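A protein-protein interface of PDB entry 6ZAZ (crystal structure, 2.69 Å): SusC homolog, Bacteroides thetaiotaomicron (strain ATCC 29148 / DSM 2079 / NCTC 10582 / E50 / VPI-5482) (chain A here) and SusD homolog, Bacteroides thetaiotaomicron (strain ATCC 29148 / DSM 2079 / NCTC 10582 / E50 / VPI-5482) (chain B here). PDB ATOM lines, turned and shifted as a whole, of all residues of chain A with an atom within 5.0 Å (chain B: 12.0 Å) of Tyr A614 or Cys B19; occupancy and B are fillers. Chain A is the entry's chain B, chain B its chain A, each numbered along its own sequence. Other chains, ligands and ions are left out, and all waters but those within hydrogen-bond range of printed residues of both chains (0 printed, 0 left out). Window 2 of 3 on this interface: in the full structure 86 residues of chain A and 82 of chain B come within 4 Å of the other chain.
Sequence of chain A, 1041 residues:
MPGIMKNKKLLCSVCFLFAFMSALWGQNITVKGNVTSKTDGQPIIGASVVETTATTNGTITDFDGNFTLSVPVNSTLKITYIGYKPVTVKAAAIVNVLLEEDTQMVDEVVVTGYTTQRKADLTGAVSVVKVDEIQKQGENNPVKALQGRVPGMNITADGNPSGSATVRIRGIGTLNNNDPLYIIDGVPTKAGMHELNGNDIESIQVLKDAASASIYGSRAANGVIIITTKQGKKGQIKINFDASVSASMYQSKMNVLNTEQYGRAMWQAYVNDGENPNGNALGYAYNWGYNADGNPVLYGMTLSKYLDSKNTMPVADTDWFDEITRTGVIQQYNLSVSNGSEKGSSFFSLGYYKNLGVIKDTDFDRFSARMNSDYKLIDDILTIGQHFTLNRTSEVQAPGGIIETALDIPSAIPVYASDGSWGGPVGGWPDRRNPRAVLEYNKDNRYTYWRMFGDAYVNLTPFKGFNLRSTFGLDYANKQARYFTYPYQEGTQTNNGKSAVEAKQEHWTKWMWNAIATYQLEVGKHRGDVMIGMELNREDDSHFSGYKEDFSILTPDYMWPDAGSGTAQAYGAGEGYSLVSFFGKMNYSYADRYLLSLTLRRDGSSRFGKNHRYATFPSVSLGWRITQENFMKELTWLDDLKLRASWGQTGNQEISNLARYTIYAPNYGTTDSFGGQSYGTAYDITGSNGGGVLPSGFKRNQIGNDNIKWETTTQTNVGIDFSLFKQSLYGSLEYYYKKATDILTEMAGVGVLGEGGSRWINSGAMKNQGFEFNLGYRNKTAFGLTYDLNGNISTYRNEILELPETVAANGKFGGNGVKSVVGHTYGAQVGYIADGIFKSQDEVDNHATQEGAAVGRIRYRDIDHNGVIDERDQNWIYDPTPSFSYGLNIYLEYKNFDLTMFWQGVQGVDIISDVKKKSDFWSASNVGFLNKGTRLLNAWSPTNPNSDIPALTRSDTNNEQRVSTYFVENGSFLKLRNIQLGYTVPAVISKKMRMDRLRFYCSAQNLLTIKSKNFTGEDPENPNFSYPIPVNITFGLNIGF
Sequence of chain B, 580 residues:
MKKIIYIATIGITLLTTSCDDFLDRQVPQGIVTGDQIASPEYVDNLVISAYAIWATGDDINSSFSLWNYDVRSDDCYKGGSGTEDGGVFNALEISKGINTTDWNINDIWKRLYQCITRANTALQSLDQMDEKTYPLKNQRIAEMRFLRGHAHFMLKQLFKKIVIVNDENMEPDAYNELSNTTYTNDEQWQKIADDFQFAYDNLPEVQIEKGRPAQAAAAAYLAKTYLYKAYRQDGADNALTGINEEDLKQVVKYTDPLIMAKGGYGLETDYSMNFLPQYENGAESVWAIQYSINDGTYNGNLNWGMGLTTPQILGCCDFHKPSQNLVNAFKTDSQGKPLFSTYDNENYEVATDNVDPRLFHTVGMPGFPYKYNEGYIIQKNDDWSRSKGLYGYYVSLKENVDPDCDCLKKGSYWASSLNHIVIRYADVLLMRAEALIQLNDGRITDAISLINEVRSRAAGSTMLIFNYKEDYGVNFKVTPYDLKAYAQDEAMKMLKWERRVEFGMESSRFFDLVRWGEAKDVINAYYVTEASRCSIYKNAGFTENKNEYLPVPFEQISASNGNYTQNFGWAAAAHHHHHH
OH of Tyr A614 sits at hydrogen-bond distance from O of Cys B19. The side-chain carboxylate (OD1) of Asp B24 lies within salt-bridge range of the guanidinium group (NH2) of Arg A613 (2.9 Å).
The side-chain carboxylate of Asp B24 sits close to the backbone carbonyl oxygen of Asp B20. O of Val A580 sits at hydrogen-bond distance from N of Gly A604 (3.0 Å). O of Arg A613 is in hydrogen-bond range of NE1 of Trp A710.
Val A580 touches Phe B22 (CG2 to CD2, 3.8 Å). Leu B23 touches Val A580 (CD1 to CG2, 3.7 Å). Leu B23 touches Gly A604. Arg A613 touches Leu B23. Tyr A614 touches Leu B23.
No residue of chain B comes within 4 Å of Arg A602. No residue of chain B comes within 4 Å of Asp A603. Of chain B, only Cys B19 (2.8 Å) and Leu B23 (3.7 Å) come within 4 Å of Tyr A614. Thr A616 touches none of the printed residues of chain B. Of the printed residues of chain A, Phe B22 touches Val A580 (3.8 Å). Of the printed residues of chain A, Leu B23 touches Val A580 (3.7 Å), Gly A604 (3.7 Å), Arg A613 (3.6 Å) and Tyr A614 (3.7 Å). Of the printed residues of chain A, Asp B24 touches Arg A613 (2.9 Å). The nearest residue of chain A that does not touch Cys B19 is Val A580 (4.2 Å). The nearest printed residue of chain A that does not touch Leu B23 is Asp A603 (6.6 Å).
Of the 8 printed residues of chain B, 4 touch a printed residue of chain A. Hydrophobic or aromatic side chains of chain B within 4 Å of the printed part of chain A: Phe B22 and Leu B23. Hydrophobic or aromatic side chains of chain A that line the printed part of chain B: Val A580 and Tyr A614. Among the printed residues, 7 pairs touch across the chains.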
ATOM      1  N   VAL A 580     -26.118  23.565   6.531  1.00  0.00           N
ATOM      2  CA  VAL A 580     -25.672  22.287   5.997  1.00  0.00           C
ATOM      3  C   VAL A 580     -26.849  21.679   5.252  1.00  0.00           C
ATOM      4  O   VAL A 580     -28.007  21.870   5.638  1.00  0.00           O
ATOM      5  CB  VAL A 580     -25.167  21.338   7.104  1.00  0.00           C
ATOM      6  CG1 VAL A 580     -24.761  20.030   6.516  1.00  0.00           C
ATOM      7  CG2 VAL A 580     -23.992  21.947   7.836  1.00  0.00           C
ATOM      8  N   PHE A 582     -28.078  18.068   2.798  1.00  0.00           N
ATOM      9  CA  PHE A 582     -27.868  16.778   2.142  1.00  0.00           C
ATOM     10  C   PHE A 582     -29.056  16.516   1.244  1.00  0.00           C
ATOM     11  O   PHE A 582     -30.205  16.675   1.677  1.00  0.00           O
ATOM     12  CB  PHE A 582     -27.711  15.657   3.169  1.00  0.00           C
ATOM     13  CG  PHE A 582     -26.674  15.952   4.193  1.00  0.00           C
ATOM     14  CD1 PHE A 582     -25.334  15.808   3.893  1.00  0.00           C
ATOM     15  CD2 PHE A 582     -27.042  16.453   5.425  1.00  0.00           C
ATOM     16  CE1 PHE A 582     -24.394  16.118   4.811  1.00  0.00           C
ATOM     17  CE2 PHE A 582     -26.103  16.766   6.348  1.00  0.00           C
ATOM     18  CZ  PHE A 582     -24.776  16.599   6.049  1.00  0.00           C
ATOM     19  N   ARG A 602     -32.329  16.802   3.521  1.00  0.00           N
ATOM     20  CA  ARG A 602     -32.270  17.007   4.960  1.00  0.00           C
ATOM     21  C   ARG A 602     -31.432  18.258   5.200  1.00  0.00           C
ATOM     22  O   ARG A 602     -30.309  18.362   4.692  1.00  0.00           O
ATOM     23  CB  ARG A 602     -31.680  15.790   5.681  1.00  0.00           C
ATOM     24  CG  ARG A 602     -31.915  15.801   7.186  1.00  0.00           C
ATOM     25  CD  ARG A 602     -31.950  14.395   7.791  1.00  0.00           C
ATOM     26  NE  ARG A 602     -31.000  14.285   8.898  1.00  0.00           N
ATOM     27  CZ  ARG A 602     -31.033  13.345   9.838  1.00  0.00           C
ATOM     28  NH1 ARG A 602     -31.983  12.415   9.815  1.00  0.00           N
ATOM     29  NH2 ARG A 602     -30.111  13.343  10.800  1.00  0.00           N
ATOM     30  N   ASP A 603     -31.982  19.209   5.962  1.00  0.00           N
ATOM     31  CA  ASP A 603     -31.525  20.594   5.956  1.00  0.00           C
ATOM     32  C   ASP A 603     -31.360  21.105   7.374  1.00  0.00           C
ATOM     33  O   ASP A 603     -32.343  21.202   8.114  1.00  0.00           O
ATOM     34  CB  ASP A 603     -32.514  21.473   5.200  1.00  0.00           C
ATOM     35  CG  ASP A 603     -32.404  21.295   3.702  1.00  0.00           C
ATOM     36  OD1 ASP A 603     -31.309  20.908   3.242  1.00  0.00           O
ATOM     37  OD2 ASP A 603     -33.397  21.539   2.968  1.00  0.00           O
ATOM     38  N   GLY A 604     -30.121  21.452   7.739  1.00  0.00           N
ATOM     39  CA  GLY A 604     -29.803  21.963   9.059  1.00  0.00           C
ATOM     40  C   GLY A 604     -29.457  23.436   8.985  1.00  0.00           C
ATOM     41  O   GLY A 604     -28.992  23.925   7.957  1.00  0.00           O
ATOM     42  N   HIS A 612     -33.616  20.666  17.241  1.00  0.00           N
ATOM     43  CA  HIS A 612     -34.459  20.936  16.073  1.00  0.00           C
ATOM     44  C   HIS A 612     -33.640  21.303  14.825  1.00  0.00           C
ATOM     45  O   HIS A 612     -34.212  21.792  13.841  1.00  0.00           O
ATOM     46  CB  HIS A 612     -35.475  22.051  16.384  1.00  0.00           C
ATOM     47  CG  HIS A 612     -36.656  21.619  17.216  1.00  0.00           C
ATOM     48  ND1 HIS A 612     -36.703  21.765  18.589  1.00  0.00           N
ATOM     49  CD2 HIS A 612     -37.852  21.088  16.864  1.00  0.00           C
ATOM     50  CE1 HIS A 612     -37.862  21.324  19.047  1.00  0.00           C
ATOM     51  NE2 HIS A 612     -38.578  20.906  18.021  1.00  0.00           N
ATOM     52  N   ARG A 613     -32.321  21.056  14.844  1.00  0.00           N
ATOM     53  CA  ARG A 613     -31.399  21.503  13.793  1.00  0.00           C
ATOM     54  C   ARG A 613     -31.921  21.244  12.393  1.00  0.00           C
ATOM     55  O   ARG A 613     -31.937  22.145  11.549  1.00  0.00           O
ATOM     56  CB  ARG A 613     -30.061  20.779  13.905  1.00  0.00           C
ATOM     57  CG  ARG A 613     -28.954  21.481  14.606  1.00  0.00           C
ATOM     58  CD  ARG A 613     -28.427  22.676  13.913  1.00  0.00           C
ATOM     59  NE  ARG A 613     -28.111  23.610  14.974  1.00  0.00           N
ATOM     60  CZ  ARG A 613     -27.065  23.501  15.778  1.00  0.00           C
ATOM     61  NH1 ARG A 613     -26.205  22.489  15.624  1.00  0.00           N
ATOM     62  NH2 ARG A 613     -26.896  24.399  16.740  1.00  0.00           N
ATOM     63  N   TYR A 614     -32.240  19.989  12.098  1.00  0.00           N
ATOM     64  CA  TYR A 614     -32.512  19.549  10.738  1.00  0.00           C
ATOM     65  C   TYR A 614     -34.003  19.327  10.507  1.00  0.00           C
ATOM     66  O   TYR A 614     -34.824  19.381  11.420  1.00  0.00           O
ATOM     67  CB  TYR A 614     -31.750  18.266  10.421  1.00  0.00           C
ATOM     68  CG  TYR A 614     -30.295  18.471  10.291  1.00  0.00           C
ATOM     69  CD1 TYR A 614     -29.486  18.545  11.426  1.00  0.00           C
ATOM     70  CD2 TYR A 614     -29.703  18.602   9.036  1.00  0.00           C
ATOM     71  CE1 TYR A 614     -28.108  18.758  11.320  1.00  0.00           C
ATOM     72  CE2 TYR A 614     -28.315  18.831   8.914  1.00  0.00           C
ATOM     73  CZ  TYR A 614     -27.531  18.905  10.065  1.00  0.00           C
ATOM     74  OH  TYR A 614     -26.175  19.114   9.965  1.00  0.00           O
ATOM     75  N   ALA A 615     -34.340  19.083   9.246  1.00  0.00           N
ATOM     76  CA  ALA A 615     -35.706  18.835   8.831  1.00  0.00           C
ATOM     77  C   ALA A 615     -35.620  18.219   7.452  1.00  0.00           C
ATOM     78  O   ALA A 615     -34.599  18.343   6.778  1.00  0.00           O
ATOM     79  CB  ALA A 615     -36.549  20.105   8.844  1.00  0.00           C
ATOM     80  N   THR A 616     -36.672  17.501   7.059  1.00  0.00           N
ATOM     81  CA  THR A 616     -36.577  16.610   5.908  1.00  0.00           C
ATOM     82  C   THR A 616     -37.710  16.903   4.948  1.00  0.00           C
ATOM     83  O   THR A 616     -38.885  16.891   5.336  1.00  0.00           O
ATOM     84  CB  THR A 616     -36.604  15.137   6.323  1.00  0.00           C
ATOM     85  OG1 THR A 616     -35.462  14.858   7.126  1.00  0.00           O
ATOM     86  CG2 THR A 616     -36.557  14.249   5.102  1.00  0.00           C
ATOM     87  N   TRP A 710     -37.787  24.229  11.877  1.00  0.00           N
ATOM     88  CA  TRP A 710     -38.041  24.678  10.520  1.00  0.00           C
ATOM     89  C   TRP A 710     -39.515  24.981  10.298  1.00  0.00           C
ATOM     90  O   TRP A 710     -40.391  24.198  10.682  1.00  0.00           O
ATOM     91  CB  TRP A 710     -37.584  23.613   9.531  1.00  0.00           C
ATOM     92  CG  TRP A 710     -36.129  23.547   9.416  1.00  0.00           C
ATOM     93  CD1 TRP A 710     -35.275  22.956  10.284  1.00  0.00           C
ATOM     94  CD2 TRP A 710     -35.332  24.104   8.374  1.00  0.00           C
ATOM     95  NE1 TRP A 710     -33.980  23.101   9.848  1.00  0.00           N
ATOM     96  CE2 TRP A 710     -33.986  23.806   8.676  1.00  0.00           C
ATOM     97  CE3 TRP A 710     -35.621  24.829   7.214  1.00  0.00           C
ATOM     98  CZ2 TRP A 710     -32.931  24.203   7.863  1.00  0.00           C
ATOM     99  CZ3 TRP A 710     -34.567  25.225   6.403  1.00  0.00           C
ATOM    100  CH2 TRP A 710     -33.239  24.915   6.734  1.00  0.00           C
ATOM    101  N   CYS B  19     -21.403  19.000   9.390  1.00  0.00           N
ATOM    102  CA  CYS B  19     -22.495  18.256  10.021  1.00  0.00           C
ATOM    103  C   CYS B  19     -22.891  18.763  11.437  1.00  0.00           C
ATOM    104  O   CYS B  19     -24.081  18.796  11.775  1.00  0.00           O
ATOM    105  CB  CYS B  19     -22.141  16.748  10.080  1.00  0.00           C
ATOM    106  SG  CYS B  19     -21.318  16.053  11.602  1.00  0.00           S
ATOM    107  N   ASP B  20     -21.909  19.146  12.264  1.00  0.00           N
ATOM    108  CA  ASP B  20     -22.196  19.429  13.672  1.00  0.00           C
ATOM    109  C   ASP B  20     -21.340  20.570  14.216  1.00  0.00           C
ATOM    110  O   ASP B  20     -21.884  21.586  14.665  1.00  0.00           O
ATOM    111  CB  ASP B  20     -22.001  18.163  14.529  1.00  0.00           C
ATOM    112  CG  ASP B  20     -23.044  18.025  15.656  1.00  0.00           C
ATOM    113  OD1 ASP B  20     -23.563  19.056  16.146  1.00  0.00           O
ATOM    114  OD2 ASP B  20     -23.333  16.874  16.063  1.00  0.00           O
ATOM    115  N   ASP B  21     -20.006  20.415  14.201  1.00  0.00           N
ATOM    116  CA  ASP B  21     -19.149  21.489  14.694  1.00  0.00           C
ATOM    117  C   ASP B  21     -19.350  22.776  13.893  1.00  0.00           C
ATOM    118  O   ASP B  21     -19.238  23.884  14.437  1.00  0.00           O
ATOM    119  CB  ASP B  21     -17.688  21.054  14.646  1.00  0.00           C
ATOM    120  CG  ASP B  21     -16.738  22.208  14.917  1.00  0.00           C
ATOM    121  OD1 ASP B  21     -16.929  22.913  15.936  1.00  0.00           O
ATOM    122  OD2 ASP B  21     -15.823  22.437  14.094  1.00  0.00           O
ATOM    123  N   PHE B  22     -19.699  22.636  12.615  1.00  0.00           N
ATOM    124  CA  PHE B  22     -19.866  23.752  11.696  1.00  0.00           C
ATOM    125  C   PHE B  22     -21.053  24.661  12.051  1.00  0.00           C
ATOM    126  O   PHE B  22     -20.976  25.880  11.852  1.00  0.00           O
ATOM    127  CB  PHE B  22     -20.013  23.150  10.300  1.00  0.00           C
ATOM    128  CG  PHE B  22     -20.104  24.140   9.183  1.00  0.00           C
ATOM    129  CD1 PHE B  22     -18.958  24.615   8.572  1.00  0.00           C
ATOM    130  CD2 PHE B  22     -21.338  24.532   8.690  1.00  0.00           C
ATOM    131  CE1 PHE B  22     -19.035  25.495   7.522  1.00  0.00           C
ATOM    132  CE2 PHE B  22     -21.423  25.416   7.633  1.00  0.00           C
ATOM    133  CZ  PHE B  22     -20.271  25.901   7.049  1.00  0.00           C
ATOM    134  N   LEU B  23     -22.162  24.115  12.537  1.00  0.00           N
ATOM    135  CA  LEU B  23     -23.338  24.927  12.807  1.00  0.00           C
ATOM    136  C   LEU B  23     -23.385  25.428  14.228  1.00  0.00           C
ATOM    137  O   LEU B  23     -24.440  25.922  14.654  1.00  0.00           O
ATOM    138  CB  LEU B  23     -24.633  24.157  12.532  1.00  0.00           C
ATOM    139  CG  LEU B  23     -24.783  23.409  11.223  1.00  0.00           C
ATOM    140  CD1 LEU B  23     -24.397  21.975  11.473  1.00  0.00           C
ATOM    141  CD2 LEU B  23     -26.209  23.503  10.725  1.00  0.00           C
ATOM    142  N   ASP B  24     -22.280  25.320  14.973  1.00  0.00           N
ATOM    143  CA  ASP B  24     -22.205  25.881  16.317  1.00  0.00           C
ATOM    144  C   ASP B  24     -21.166  26.978  16.472  1.00  0.00           C
ATOM    145  O   ASP B  24     -21.176  27.660  17.506  1.00  0.00           O
ATOM    146  CB  ASP B  24     -21.910  24.782  17.348  1.00  0.00           C
ATOM    147  CG  ASP B  24     -22.984  23.707  17.384  1.00  0.00           C
ATOM    148  OD1 ASP B  24     -24.149  24.044  17.727  1.00  0.00           O
ATOM    149  OD2 ASP B  24     -22.651  22.534  17.068  1.00  0.00           O
ATOM    150  N   ARG B  25     -20.290  27.176  15.476  1.00  0.00           N
ATOM    151  CA  ARG B  25     -19.139  28.062  15.631  1.00  0.00           C
ATOM    152  C   ARG B  25     -19.567  29.504  15.868  1.00  0.00           C
ATOM    153  O   ARG B  25     -19.130  30.134  16.837  1.00  0.00           O
ATOM    154  CB  ARG B  25     -18.232  27.964  14.406  1.00  0.00           C
ATOM    155  CG  ARG B  25     -17.164  26.889  14.537  1.00  0.00           C
ATOM    156  CD  ARG B  25     -15.946  27.150  13.654  1.00  0.00           C
ATOM    157  NE  ARG B  25     -15.449  25.907  13.058  1.00  0.00           N
ATOM    158  CZ  ARG B  25     -15.863  25.414  11.890  1.00  0.00           C
ATOM    159  NH1 ARG B  25     -16.774  26.066  11.182  1.00  0.00           N
ATOM    160  NH2 ARG B  25     -15.363  24.271  11.422  1.00  0.00           N
ATOM    161  N   GLN B  26     -20.431  30.042  15.004  1.00  0.00           N
ATOM    162  CA  GLN B  26     -20.845  31.436  15.128  1.00  0.00           C
ATOM    163  C   GLN B  26     -21.826  31.601  16.274  1.00  0.00           C
ATOM    164  O   GLN B  26     -22.762  30.810  16.422  1.00  0.00           O
ATOM    165  CB  GLN B  26     -21.458  31.920  13.822  1.00  0.00           C
ATOM    166  CG  GLN B  26     -20.650  31.459  12.626  1.00  0.00           C
ATOM    167  CD  GLN B  26     -21.457  31.369  11.367  1.00  0.00           C
ATOM    168  OE1 GLN B  26     -22.280  30.473  11.209  1.00  0.00           O
ATOM    169  NE2 GLN B  26     -21.228  32.303  10.454  1.00  0.00           N
